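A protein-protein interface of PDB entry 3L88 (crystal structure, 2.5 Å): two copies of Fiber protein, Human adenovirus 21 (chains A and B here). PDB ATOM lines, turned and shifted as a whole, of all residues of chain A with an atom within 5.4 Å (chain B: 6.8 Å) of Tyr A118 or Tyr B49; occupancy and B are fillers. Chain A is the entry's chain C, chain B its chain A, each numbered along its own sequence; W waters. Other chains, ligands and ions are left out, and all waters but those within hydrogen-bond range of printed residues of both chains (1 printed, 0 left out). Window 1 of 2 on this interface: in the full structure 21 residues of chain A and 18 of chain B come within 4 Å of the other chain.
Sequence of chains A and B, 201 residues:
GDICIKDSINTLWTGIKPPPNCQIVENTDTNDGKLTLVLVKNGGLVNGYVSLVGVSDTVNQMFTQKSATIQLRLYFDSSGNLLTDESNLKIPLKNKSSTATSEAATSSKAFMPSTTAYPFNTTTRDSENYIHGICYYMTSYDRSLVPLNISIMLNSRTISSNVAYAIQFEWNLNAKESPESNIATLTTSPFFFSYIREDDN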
ATOM      1  N   LEU A  45      -0.902  -7.780  27.380  1.00  0.00           N
ATOM      2  CA  LEU A  45      -1.692  -8.940  27.745  1.00  0.00           C
ATOM      3  C   LEU A  45      -3.161  -8.661  27.765  1.00  0.00           C
ATOM      4  O   LEU A  45      -3.587  -7.535  27.796  1.00  0.00           O
ATOM      5  CB  LEU A  45      -1.323  -9.446  29.124  1.00  0.00           C
ATOM      6  CG  LEU A  45       0.138  -9.564  29.439  1.00  0.00           C
ATOM      7  CD1 LEU A  45       0.317  -9.412  30.918  1.00  0.00           C
ATOM      8  CD2 LEU A  45       0.627 -10.892  28.967  1.00  0.00           C
ATOM      9  N   PRO A 113      -6.182 -14.077  21.579  1.00  0.00           N
ATOM     10  CA  PRO A 113      -4.872 -14.662  21.870  1.00  0.00           C
ATOM     11  C   PRO A 113      -3.955 -14.599  20.651  1.00  0.00           C
ATOM     12  O   PRO A 113      -4.351 -14.992  19.559  1.00  0.00           O
ATOM     13  CB  PRO A 113      -5.202 -16.119  22.215  1.00  0.00           C
ATOM     14  CG  PRO A 113      -6.526 -16.376  21.578  1.00  0.00           C
ATOM     15  CD  PRO A 113      -7.264 -15.074  21.605  1.00  0.00           C
ATOM     16  N   SER A 114      -2.739 -14.103  20.847  1.00  0.00           N
ATOM     17  CA  SER A 114      -1.797 -13.905  19.752  1.00  0.00           C
ATOM     18  C   SER A 114      -1.501 -15.192  18.998  1.00  0.00           C
ATOM     19  O   SER A 114      -1.170 -16.218  19.592  1.00  0.00           O
ATOM     20  CB  SER A 114      -0.493 -13.293  20.264  1.00  0.00           C
ATOM     21  OG  SER A 114       0.546 -13.442  19.308  1.00  0.00           O
ATOM     22  N   THR A 115      -1.580 -15.111  17.677  1.00  0.00           N
ATOM     23  CA  THR A 115      -1.304 -16.246  16.816  1.00  0.00           C
ATOM     24  C   THR A 115       0.193 -16.532  16.721  1.00  0.00           C
ATOM     25  O   THR A 115       0.603 -17.628  16.331  1.00  0.00           O
ATOM     26  CB  THR A 115      -1.874 -16.010  15.409  1.00  0.00           C
ATOM     27  OG1 THR A 115      -3.277 -16.286  15.415  1.00  0.00           O
ATOM     28  CG2 THR A 115      -1.192 -16.911  14.403  1.00  0.00           C
ATOM     29  N   THR A 116       1.002 -15.540  17.077  1.00  0.00           N
ATOM     30  CA  THR A 116       2.447 -15.723  17.150  1.00  0.00           C
ATOM     31  C   THR A 116       2.833 -16.486  18.410  1.00  0.00           C
ATOM     32  O   THR A 116       3.565 -17.474  18.346  1.00  0.00           O
ATOM     33  CB  THR A 116       3.200 -14.378  17.102  1.00  0.00           C
ATOM     34  OG1 THR A 116       2.822 -13.655  15.924  1.00  0.00           O
ATOM     35  CG2 THR A 116       4.705 -14.609  17.082  1.00  0.00           C
ATOM     36  N   ALA A 117       2.320 -16.042  19.552  1.00  0.00           N
ATOM     37  CA  ALA A 117       2.657 -16.666  20.827  1.00  0.00           C
ATOM     38  C   ALA A 117       1.985 -18.029  20.971  1.00  0.00           C
ATOM     39  O   ALA A 117       2.562 -18.964  21.532  1.00  0.00           O
ATOM     40  CB  ALA A 117       2.276 -15.757  21.980  1.00  0.00           C
ATOM     41  N   TYR A 118       0.764 -18.134  20.453  1.00  0.00           N
ATOM     42  CA  TYR A 118       0.002 -19.372  20.517  1.00  0.00           C
ATOM     43  C   TYR A 118      -0.499 -19.742  19.126  1.00  0.00           C
ATOM     44  O   TYR A 118      -1.626 -19.417  18.753  1.00  0.00           O
ATOM     45  CB  TYR A 118      -1.174 -19.233  21.490  1.00  0.00           C
ATOM     46  CG  TYR A 118      -0.852 -18.430  22.735  1.00  0.00           C
ATOM     47  CD1 TYR A 118      -0.070 -18.970  23.753  1.00  0.00           C
ATOM     48  CD2 TYR A 118      -1.312 -17.125  22.880  1.00  0.00           C
ATOM     49  CE1 TYR A 118       0.233 -18.238  24.892  1.00  0.00           C
ATOM     50  CE2 TYR A 118      -1.020 -16.386  24.017  1.00  0.00           C
ATOM     51  CZ  TYR A 118      -0.249 -16.948  25.020  1.00  0.00           C
ATOM     52  OH  TYR A 118       0.049 -16.210  26.142  1.00  0.00           O
ATOM     53  N   PRO A 119       0.348 -20.424  18.347  1.00  0.00           N
ATOM     54  CA  PRO A 119       0.043 -20.715  16.954  1.00  0.00           C
ATOM     55  C   PRO A 119      -0.896 -21.906  16.795  1.00  0.00           C
ATOM     56  O   PRO A 119      -1.000 -22.742  17.689  1.00  0.00           O
ATOM     57  CB  PRO A 119       1.414 -21.042  16.361  1.00  0.00           C
ATOM     58  CG  PRO A 119       2.189 -21.613  17.503  1.00  0.00           C
ATOM     59  CD  PRO A 119       1.649 -20.982  18.764  1.00  0.00           C
ATOM     60  N   PHE A 120      -1.577 -21.973  15.657  1.00  0.00           N
ATOM     61  CA  PHE A 120      -2.284 -23.181  15.259  1.00  0.00           C
ATOM     62  C   PHE A 120      -1.287 -24.230  14.761  1.00  0.00           C
ATOM     63  O   PHE A 120      -0.369 -23.915  14.000  1.00  0.00           O
ATOM     64  CB  PHE A 120      -3.316 -22.860  14.175  1.00  0.00           C
ATOM     65  CG  PHE A 120      -4.459 -21.998  14.654  1.00  0.00           C
ATOM     66  CD1 PHE A 120      -5.580 -22.567  15.228  1.00  0.00           C
ATOM     67  CD2 PHE A 120      -4.421 -20.620  14.504  1.00  0.00           C
ATOM     68  CE1 PHE A 120      -6.642 -21.777  15.643  1.00  0.00           C
ATOM     69  CE2 PHE A 120      -5.477 -19.824  14.923  1.00  0.00           C
ATOM     70  CZ  PHE A 120      -6.584 -20.405  15.497  1.00  0.00           C
ATOM     71  N   GLU A 128       2.761 -25.475  24.803  1.00  0.00           N
ATOM     72  CA  GLU A 128       2.914 -24.038  24.998  1.00  0.00           C
ATOM     73  C   GLU A 128       1.627 -23.262  24.741  1.00  0.00           C
ATOM     74  O   GLU A 128       1.578 -22.048  24.948  1.00  0.00           O
ATOM     75  CB  GLU A 128       4.034 -23.487  24.115  1.00  0.00           C
ATOM     76  CG  GLU A 128       5.423 -23.792  24.626  1.00  0.00           C
ATOM     77  CD  GLU A 128       6.452 -23.801  23.517  1.00  0.00           C
ATOM     78  OE1 GLU A 128       6.614 -22.757  22.848  1.00  0.00           O
ATOM     79  OE2 GLU A 128       7.093 -24.855  23.313  1.00  0.00           O
ATOM     80  N   ASN A 129       0.591 -23.961  24.288  1.00  0.00           N
ATOM     81  CA  ASN A 129      -0.695 -23.326  24.013  1.00  0.00           C
ATOM     82  C   ASN A 129      -1.638 -23.398  25.208  1.00  0.00           C
ATOM     83  O   ASN A 129      -2.769 -22.913  25.154  1.00  0.00           O
ATOM     84  CB  ASN A 129      -1.366 -23.966  22.798  1.00  0.00           C
ATOM     85  CG  ASN A 129      -0.656 -23.650  21.508  1.00  0.00           C
ATOM     86  OD1 ASN A 129       0.500 -24.024  21.318  1.00  0.00           O
ATOM     87  ND2 ASN A 129      -1.353 -22.974  20.598  1.00  0.00           N
ATOM     88  N   ILE A 131      -2.833 -22.986  29.273  1.00  0.00           N
ATOM     89  CA  ILE A 131      -2.756 -22.490  30.641  1.00  0.00           C
ATOM     90  C   ILE A 131      -3.413 -23.492  31.581  1.00  0.00           C
ATOM     91  O   ILE A 131      -4.460 -24.056  31.267  1.00  0.00           O
ATOM     92  CB  ILE A 131      -3.450 -21.125  30.795  1.00  0.00           C
ATOM     93  CG1 ILE A 131      -2.699 -20.046  30.010  1.00  0.00           C
ATOM     94  CG2 ILE A 131      -3.562 -20.744  32.263  1.00  0.00           C
ATOM     95  CD1 ILE A 131      -3.522 -18.794  29.768  1.00  0.00           C
ATOM     96  N   LEU A 154      -5.216 -22.123  24.028  1.00  0.00           N
ATOM     97  CA  LEU A 154      -5.307 -20.986  23.120  1.00  0.00           C
ATOM     98  C   LEU A 154      -4.980 -21.379  21.682  1.00  0.00           C
ATOM     99  O   LEU A 154      -3.945 -21.999  21.409  1.00  0.00           O
ATOM    100  CB  LEU A 154      -4.397 -19.849  23.589  1.00  0.00           C
ATOM    101  CG  LEU A 154      -4.701 -19.278  24.975  1.00  0.00           C
ATOM    102  CD1 LEU A 154      -3.632 -18.280  25.372  1.00  0.00           C
ATOM    103  CD2 LEU A 154      -6.083 -18.644  25.019  1.00  0.00           C
ATOM    104  N   ASN A 155      -5.881 -21.024  20.770  1.00  0.00           N
ATOM    105  CA  ASN A 155      -5.708 -21.333  19.360  1.00  0.00           C
ATOM    106  C   ASN A 155      -5.426 -22.813  19.129  1.00  0.00           C
ATOM    107  O   ASN A 155      -6.267 -23.666  19.418  1.00  0.00           O
ATOM    108  CB  ASN A 155      -4.607 -20.460  18.760  1.00  0.00           C
ATOM    109  CG  ASN A 155      -4.959 -18.979  18.795  1.00  0.00           C
ATOM    110  OD1 ASN A 155      -6.132 -18.604  18.715  1.00  0.00           O
ATOM    111  ND2 ASN A 155      -3.947 -18.131  18.928  1.00  0.00           N
ATOM    112  N   SER A 156      -4.248 -23.115  18.598  1.00  0.00           N
ATOM    113  CA  SER A 156      -3.815 -24.501  18.424  1.00  0.00           C
ATOM    114  C   SER A 156      -4.642 -25.299  17.409  1.00  0.00           C
ATOM    115  O   SER A 156      -4.086 -26.011  16.577  1.00  0.00           O
ATOM    116  CB  SER A 156      -3.786 -25.234  19.763  1.00  0.00           C
ATOM    117  OG  SER A 156      -3.544 -26.617  19.564  1.00  0.00           O
ATOM    118  N   SER A 194      -3.965 -14.693  32.361  1.00  0.00           N
ATOM    119  CA  SER A 194      -3.499 -13.725  31.380  1.00  0.00           C
ATOM    120  C   SER A 194      -2.992 -14.483  30.166  1.00  0.00           C
ATOM    121  O   SER A 194      -2.630 -15.657  30.267  1.00  0.00           O
ATOM    122  CB  SER A 194      -2.366 -12.869  31.955  1.00  0.00           C
ATOM    123  OG  SER A 194      -2.821 -12.051  33.018  1.00  0.00           O
ATOM    124  N   TYR A 195      -2.984 -13.815  29.019  1.00  0.00           N
ATOM    125  CA  TYR A 195      -2.267 -14.313  27.860  1.00  0.00           C
ATOM    126  C   TYR A 195      -1.833 -13.171  26.968  1.00  0.00           C
ATOM    127  O   TYR A 195      -2.359 -12.062  27.062  1.00  0.00           O
ATOM    128  CB  TYR A 195      -3.108 -15.322  27.078  1.00  0.00           C
ATOM    129  CG  TYR A 195      -4.432 -14.792  26.562  1.00  0.00           C
ATOM    130  CD1 TYR A 195      -4.479 -13.869  25.524  1.00  0.00           C
ATOM    131  CD2 TYR A 195      -5.639 -15.269  27.066  1.00  0.00           C
ATOM    132  CE1 TYR A 195      -5.686 -13.401  25.039  1.00  0.00           C
ATOM    133  CE2 TYR A 195      -6.850 -14.815  26.580  1.00  0.00           C
ATOM    134  CZ  TYR A 195      -6.867 -13.890  25.563  1.00  0.00           C
ATOM    135  OH  TYR A 195      -8.066 -13.437  25.084  1.00  0.00           O
ATOM    136  N   ILE A 196      -0.842 -13.439  26.127  1.00  0.00           N
ATOM    137  CA  ILE A 196      -0.327 -12.435  25.211  1.00  0.00           C
ATOM    138  C   ILE A 196      -1.330 -12.206  24.088  1.00  0.00           C
ATOM    139  O   ILE A 196      -1.747 -13.152  23.424  1.00  0.00           O
ATOM    140  CB  ILE A 196       1.025 -12.863  24.631  1.00  0.00           C
ATOM    141  CG1 ILE A 196       2.038 -13.056  25.762  1.00  0.00           C
ATOM    142  CG2 ILE A 196       1.514 -11.835  23.631  1.00  0.00           C
ATOM    143  CD1 ILE A 196       3.199 -13.964  25.414  1.00  0.00           C
ATOM    144  N   ILE B  16       7.679 -11.768  22.129  1.00  0.00           N
ATOM    145  CA  ILE B  16       6.961 -13.024  21.958  1.00  0.00           C
ATOM    146  C   ILE B  16       7.864 -14.062  21.299  1.00  0.00           C
ATOM    147  O   ILE B  16       8.561 -13.766  20.328  1.00  0.00           O
ATOM    148  CB  ILE B  16       5.695 -12.836  21.104  1.00  0.00           C
ATOM    149  CG1 ILE B  16       4.749 -11.830  21.758  1.00  0.00           C
ATOM    150  CG2 ILE B  16       4.987 -14.161  20.892  1.00  0.00           C
ATOM    151  CD1 ILE B  16       3.522 -11.513  20.919  1.00  0.00           C
ATOM    152  N   LYS B  17       7.859 -15.277  21.837  1.00  0.00           N
ATOM    153  CA  LYS B  17       8.571 -16.382  21.208  1.00  0.00           C
ATOM    154  C   LYS B  17      10.022 -15.997  20.940  1.00  0.00           C
ATOM    155  O   LYS B  17      10.466 -15.979  19.792  1.00  0.00           O
ATOM    156  CB  LYS B  17       7.877 -16.773  19.899  1.00  0.00           C
ATOM    157  CG  LYS B  17       7.787 -18.277  19.657  1.00  0.00           C
ATOM    158  CD  LYS B  17       6.629 -18.913  20.426  1.00  0.00           C
ATOM    159  CE  LYS B  17       6.426 -20.367  20.002  1.00  0.00           C
ATOM    160  NZ  LYS B  17       5.411 -21.063  20.840  1.00  0.00           N
ATOM    161  N   THR B  36      10.019 -16.581  28.529  1.00  0.00           N
ATOM    162  CA  THR B  36       9.004 -15.595  28.177  1.00  0.00           C
ATOM    163  C   THR B  36       8.530 -14.884  29.433  1.00  0.00           C
ATOM    164  O   THR B  36       8.024 -15.520  30.361  1.00  0.00           O
ATOM    165  CB  THR B  36       7.795 -16.245  27.478  1.00  0.00           C
ATOM    166  OG1 THR B  36       8.219 -16.863  26.258  1.00  0.00           O
ATOM    167  CG2 THR B  36       6.736 -15.203  27.163  1.00  0.00           C
ATOM    168  N   LEU B  37       8.724 -13.570  29.468  1.00  0.00           N
ATOM    169  CA  LEU B  37       8.352 -12.765  30.622  1.00  0.00           C
ATOM    170  C   LEU B  37       7.677 -11.480  30.175  1.00  0.00           C
ATOM    171  O   LEU B  37       8.217 -10.732  29.363  1.00  0.00           O
ATOM    172  CB  LEU B  37       9.587 -12.441  31.467  1.00  0.00           C
ATOM    173  CG  LEU B  37       9.383 -11.496  32.655  1.00  0.00           C
ATOM    174  CD1 LEU B  37       8.511 -12.144  33.716  1.00  0.00           C
ATOM    175  CD2 LEU B  37      10.737 -11.105  33.235  1.00  0.00           C
ATOM    176  N   VAL B  38       6.484 -11.233  30.700  1.00  0.00           N
ATOM    177  CA  VAL B  38       5.763 -10.002  30.404  1.00  0.00           C
ATOM    178  C   VAL B  38       5.429  -9.243  31.691  1.00  0.00           C
ATOM    179  O   VAL B  38       4.866  -9.805  32.628  1.00  0.00           O
ATOM    180  CB  VAL B  38       4.476 -10.291  29.612  1.00  0.00           C
ATOM    181  CG1 VAL B  38       3.872  -8.998  29.080  1.00  0.00           C
ATOM    182  CG2 VAL B  38       4.765 -11.253  28.471  1.00  0.00           C
ATOM    183  N   LEU B  39       5.815  -7.973  31.746  1.00  0.00           N
ATOM    184  CA  LEU B  39       5.503  -7.132  32.895  1.00  0.00           C
ATOM    185  C   LEU B  39       4.669  -5.941  32.457  1.00  0.00           C
ATOM    186  O   LEU B  39       5.099  -5.158  31.610  1.00  0.00           O
ATOM    187  CB  LEU B  39       6.783  -6.636  33.564  1.00  0.00           C
ATOM    188  CG  LEU B  39       7.777  -7.701  34.025  1.00  0.00           C
ATOM    189  CD1 LEU B  39       9.074  -7.049  34.500  1.00  0.00           C
ATOM    190  CD2 LEU B  39       7.164  -8.566  35.115  1.00  0.00           C
ATOM    191  N   VAL B  40       3.485  -5.798  33.046  1.00  0.00           N
ATOM    192  CA  VAL B  40       2.564  -4.740  32.659  1.00  0.00           C
ATOM    193  C   VAL B  40       2.230  -3.814  33.822  1.00  0.00           C
ATOM    194  O   VAL B  40       1.804  -4.266  34.884  1.00  0.00           O
ATOM    195  CB  VAL B  40       1.262  -5.315  32.088  1.00  0.00           C
ATOM    196  CG1 VAL B  40       0.274  -4.197  31.792  1.00  0.00           C
ATOM    197  CG2 VAL B  40       1.550  -6.116  30.835  1.00  0.00           C
ATOM    198  N   ASN B  47       1.479  -6.353  36.643  1.00  0.00           N
ATOM    199  CA  ASN B  47       0.927  -7.666  36.320  1.00  0.00           C
ATOM    200  C   ASN B  47       1.921  -8.491  35.514  1.00  0.00           C
ATOM    201  O   ASN B  47       2.413  -8.041  34.480  1.00  0.00           O
ATOM    202  CB  ASN B  47      -0.379  -7.535  35.530  1.00  0.00           C
ATOM    203  CG  ASN B  47      -1.584  -7.320  36.421  1.00  0.00           C
ATOM    204  OD1 ASN B  47      -1.477  -7.294  37.647  1.00  0.00           O
ATOM    205  ND2 ASN B  47      -2.742  -7.157  35.803  1.00  0.00           N
ATOM    206  N   GLY B  48       2.191  -9.707  35.976  1.00  0.00           N
ATOM    207  CA  GLY B  48       3.287 -10.499  35.444  1.00  0.00           C
ATOM    208  C   GLY B  48       2.851 -11.808  34.817  1.00  0.00           C
ATOM    209  O   GLY B  48       1.850 -12.400  35.217  1.00  0.00           O
ATOM    210  N   TYR B  49       3.643 -12.275  33.859  1.00  0.00           N
ATOM    211  CA  TYR B  49       3.370 -13.504  33.125  1.00  0.00           C
ATOM    212  C   TYR B  49       4.723 -14.116  32.786  1.00  0.00           C
ATOM    213  O   TYR B  49       5.594 -13.438  32.246  1.00  0.00           O
ATOM    214  CB  TYR B  49       2.581 -13.175  31.847  1.00  0.00           C
ATOM    215  CG  TYR B  49       2.366 -14.321  30.875  1.00  0.00           C
ATOM    216  CD1 TYR B  49       3.427 -14.866  30.162  1.00  0.00           C
ATOM    217  CD2 TYR B  49       1.088 -14.789  30.599  1.00  0.00           C
ATOM    218  CE1 TYR B  49       3.229 -15.882  29.248  1.00  0.00           C
ATOM    219  CE2 TYR B  49       0.877 -15.810  29.687  1.00  0.00           C
ATOM    220  CZ  TYR B  49       1.950 -16.349  29.008  1.00  0.00           C
ATOM    221  OH  TYR B  49       1.748 -17.367  28.095  1.00  0.00           O
ATOM    222  N   VAL B  50       4.923 -15.371  33.166  1.00  0.00           N
ATOM    223  CA  VAL B  50       6.228 -16.008  33.013  1.00  0.00           C
ATOM    224  C   VAL B  50       6.104 -17.491  32.671  1.00  0.00           C
ATOM    225  O   VAL B  50       5.373 -18.235  33.326  1.00  0.00           O
ATOM    226  CB  VAL B  50       7.091 -15.845  34.281  1.00  0.00           C
ATOM    227  CG1 VAL B  50       6.513 -16.655  35.422  1.00  0.00           C
ATOM    228  CG2 VAL B  50       8.536 -16.253  34.006  1.00  0.00           C
ATOM    229  N   SER B  51       6.813 -17.906  31.626  1.00  0.00           N
ATOM    230  CA  SER B  51       6.889 -19.313  31.248  1.00  0.00           C
ATOM    231  C   SER B  51       8.244 -19.624  30.621  1.00  0.00           C
ATOM    232  O   SER B  51       8.906 -18.736  30.077  1.00  0.00           O
ATOM    233  CB  SER B  51       5.764 -19.668  30.276  1.00  0.00           C
ATOM    234  OG  SER B  51       5.923 -18.996  29.041  1.00  0.00           O
ATOM    235  N   PHE B 169      13.314 -16.063  39.743  1.00  0.00           N
ATOM    236  CA  PHE B 169      12.368 -17.149  39.518  1.00  0.00           C
ATOM    237  C   PHE B 169      12.998 -18.495  39.862  1.00  0.00           C
ATOM    238  O   PHE B 169      14.146 -18.769  39.497  1.00  0.00           O
ATOM    239  CB  PHE B 169      11.908 -17.160  38.061  1.00  0.00           C
ATOM    240  CG  PHE B 169      11.297 -15.864  37.607  1.00  0.00           C
ATOM    241  CD1 PHE B 169       9.963 -15.588  37.854  1.00  0.00           C
ATOM    242  CD2 PHE B 169      12.056 -14.930  36.921  1.00  0.00           C
ATOM    243  CE1 PHE B 169       9.400 -14.397  37.433  1.00  0.00           C
ATOM    244  CE2 PHE B 169      11.501 -13.742  36.497  1.00  0.00           C
ATOM    245  CZ  PHE B 169      10.172 -13.472  36.758  1.00  0.00           C
ATOM    246  N   SER B 189       4.077 -24.252  32.251  1.00  0.00           N
ATOM    247  CA  SER B 189       2.865 -23.504  31.952  1.00  0.00           C
ATOM    248  C   SER B 189       2.933 -22.112  32.571  1.00  0.00           C
ATOM    249  O   SER B 189       3.570 -21.921  33.602  1.00  0.00           O
ATOM    250  CB  SER B 189       1.617 -24.265  32.413  1.00  0.00           C
ATOM    251  OG  SER B 189       1.576 -24.406  33.821  1.00  0.00           O
ATOM    252  N   PRO B 190       2.312 -21.123  31.914  1.00  0.00           N
ATOM    253  CA  PRO B 190       2.436 -19.732  32.336  1.00  0.00           C
ATOM    254  C   PRO B 190       2.012 -19.538  33.784  1.00  0.00           C
ATOM    255  O   PRO B 190       0.994 -20.067  34.207  1.00  0.00           O
ATOM    256  CB  PRO B 190       1.467 -18.995  31.408  1.00  0.00           C
ATOM    257  CG  PRO B 190       1.355 -19.870  30.211  1.00  0.00           C
ATOM    258  CD  PRO B 190       1.449 -21.268  30.730  1.00  0.00           C
ATOM    259  N   PHE B 191       2.804 -18.790  34.540  1.00  0.00           N
ATOM    260  CA  PHE B 191       2.444 -18.444  35.905  1.00  0.00           C
ATOM    261  C   PHE B 191       2.133 -16.953  35.996  1.00  0.00           C
ATOM    262  O   PHE B 191       2.849 -16.122  35.433  1.00  0.00           O
ATOM    263  CB  PHE B 191       3.570 -18.818  36.866  1.00  0.00           C
ATOM    264  CG  PHE B 191       3.274 -18.488  38.302  1.00  0.00           C
ATOM    265  CD1 PHE B 191       2.266 -19.148  38.986  1.00  0.00           C
ATOM    266  CD2 PHE B 191       4.003 -17.509  38.966  1.00  0.00           C
ATOM    267  CE1 PHE B 191       1.987 -18.832  40.306  1.00  0.00           C
ATOM    268  CE2 PHE B 191       3.738 -17.203  40.286  1.00  0.00           C
ATOM    269  CZ  PHE B 191       2.729 -17.861  40.955  1.00  0.00           C
ATOM    270  N   PHE B 192       1.034 -16.622  36.660  1.00  0.00           N
ATOM    271  CA  PHE B 192       0.606 -15.238  36.765  1.00  0.00           C
ATOM    272  C   PHE B 192       0.918 -14.703  38.157  1.00  0.00           C
ATOM    273  O   PHE B 192       0.794 -15.421  39.145  1.00  0.00           O
ATOM    274  CB  PHE B 192      -0.889 -15.116  36.462  1.00  0.00           C
ATOM    275  CG  PHE B 192      -1.355 -16.022  35.361  1.00  0.00           C
ATOM    276  CD1 PHE B 192      -2.333 -16.975  35.596  1.00  0.00           C
ATOM    277  CD2 PHE B 192      -0.806 -15.929  34.091  1.00  0.00           C
ATOM    278  CE1 PHE B 192      -2.764 -17.803  34.581  1.00  0.00           C
ATOM    279  CE2 PHE B 192      -1.232 -16.758  33.073  1.00  0.00           C
ATOM    280  CZ  PHE B 192      -2.206 -17.697  33.317  1.00  0.00           C
ATOM    281  N   PHE B 193       1.351 -13.451  38.226  1.00  0.00           N
ATOM    282  CA  PHE B 193       1.667 -12.831  39.502  1.00  0.00           C
ATOM    283  C   PHE B 193       1.503 -11.323  39.453  1.00  0.00           C
ATOM    284  O   PHE B 193       1.470 -10.723  38.379  1.00  0.00           O
ATOM    285  CB  PHE B 193       3.089 -13.185  39.931  1.00  0.00           C
ATOM    286  CG  PHE B 193       4.135 -12.778  38.940  1.00  0.00           C
ATOM    287  CD1 PHE B 193       4.422 -13.581  37.846  1.00  0.00           C
ATOM    288  CD2 PHE B 193       4.829 -11.593  39.097  1.00  0.00           C
ATOM    289  CE1 PHE B 193       5.383 -13.209  36.932  1.00  0.00           C
ATOM    290  CE2 PHE B 193       5.799 -11.215  38.186  1.00  0.00           C
ATOM    291  CZ  PHE B 193       6.075 -12.023  37.102  1.00  0.00           C
HETATM  292  O   HOH W   1       3.883 -23.711  21.014  1.00  0.00           O
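Of the 18 printed residues of chain B, 6 touch a printed residue of chain A.
Hydrophobic or aromatic side chains of chain A within 4 Å of the printed part of chain B: Leu A45, Ala A117, Tyr A118, Ile A131 and Ile A196.
Among the printed residues, merely in contact across the chains: Ser A194 with Phe B192, Ala A117 with Ile B16, Ile A196 with Ile B16, Ile A131 with Phe B192, Leu A45 with Val B40, Ser A194 with Tyr B49, Ala A117 with Lys B17, Leu A45 with Val B38, Thr A116 with Ile B16, Ser A114 with Ile B16, Tyr A195 with Tyr B49 and Thr A116 with Lys B17.
Water W1 lies within hydrogen-bond range of the side-chain amino group of Lys B17 (3.1 Å), the side-chain amide oxygen of Asn A129 (3.4 Å) and the side-chain carboxylate of Glu A128 (3.4 Å).
O of Tyr B49 lies within hydrogen-bond range of N of Val B38 (2.8 Å).
O of Val B40 sits at hydrogen-bond distance from N of Asn B47 (2.7 Å).
N of Thr A116 lies within hydrogen-bond range of OG of Ser A114 (3.1 Å).
ND2 of Asn A155 lies within hydrogen-bond range of O of Ser A114.
The backbone carbonyl oxygen (O) of Ile A196 sits at hydrogen-bond distance from the backbone NH (N) of Ser A114 (2.9 Å).
The backbone NH (N) of Ile A196 sits at hydrogen-bond distance from the side-chain hydroxyl (OH) of Tyr A118 (2.9 Å).
The side-chain amino group of Lys B17 lies within salt-bridge range of the side-chain carboxylate of Glu A128 (2.9 Å).
The side-chain hydroxyl (OH) of Tyr B49 lies within hydrogen-bond range of the side-chain hydroxyl (OH) of Tyr A118 (2.8 Å).
Printed residues of chain B within 4 Å of Leu A45: Val B38 (3.8 Å) and Val B40 (3.5 Å).
Printed residues of chain B within 4 Å of Thr A116: Ile B16 and Lys B17.
Of chain B, only Tyr B49 (2.8 Å) comes within 4 Å of Tyr A118.
Asn A129 touches none of the printed residues of chain B.
Of the printed residues of chain B, Ser A194 touches Tyr B49 and Phe B192.
Printed residues of chain B within 4 Å of Ile A196: Ile B16 (3.4 Å).
Of the printed residues of chain A, Val B38 touches Leu A45.
Of chain A, only Tyr A118, Ser A194 and Tyr A195 come within 4 Å of Tyr B49.
The nearest residue of chain B that does not touch Tyr A118 is Lys B17 (5.5 Å).
The nearest residue of chain A that does not touch Tyr B49 is Leu A45 (4.2 Å).
No position is printed for both chains.
Of the 14 pairs that touch across the chains among the printed residues, none has its exchanged pair printed and touching as well.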
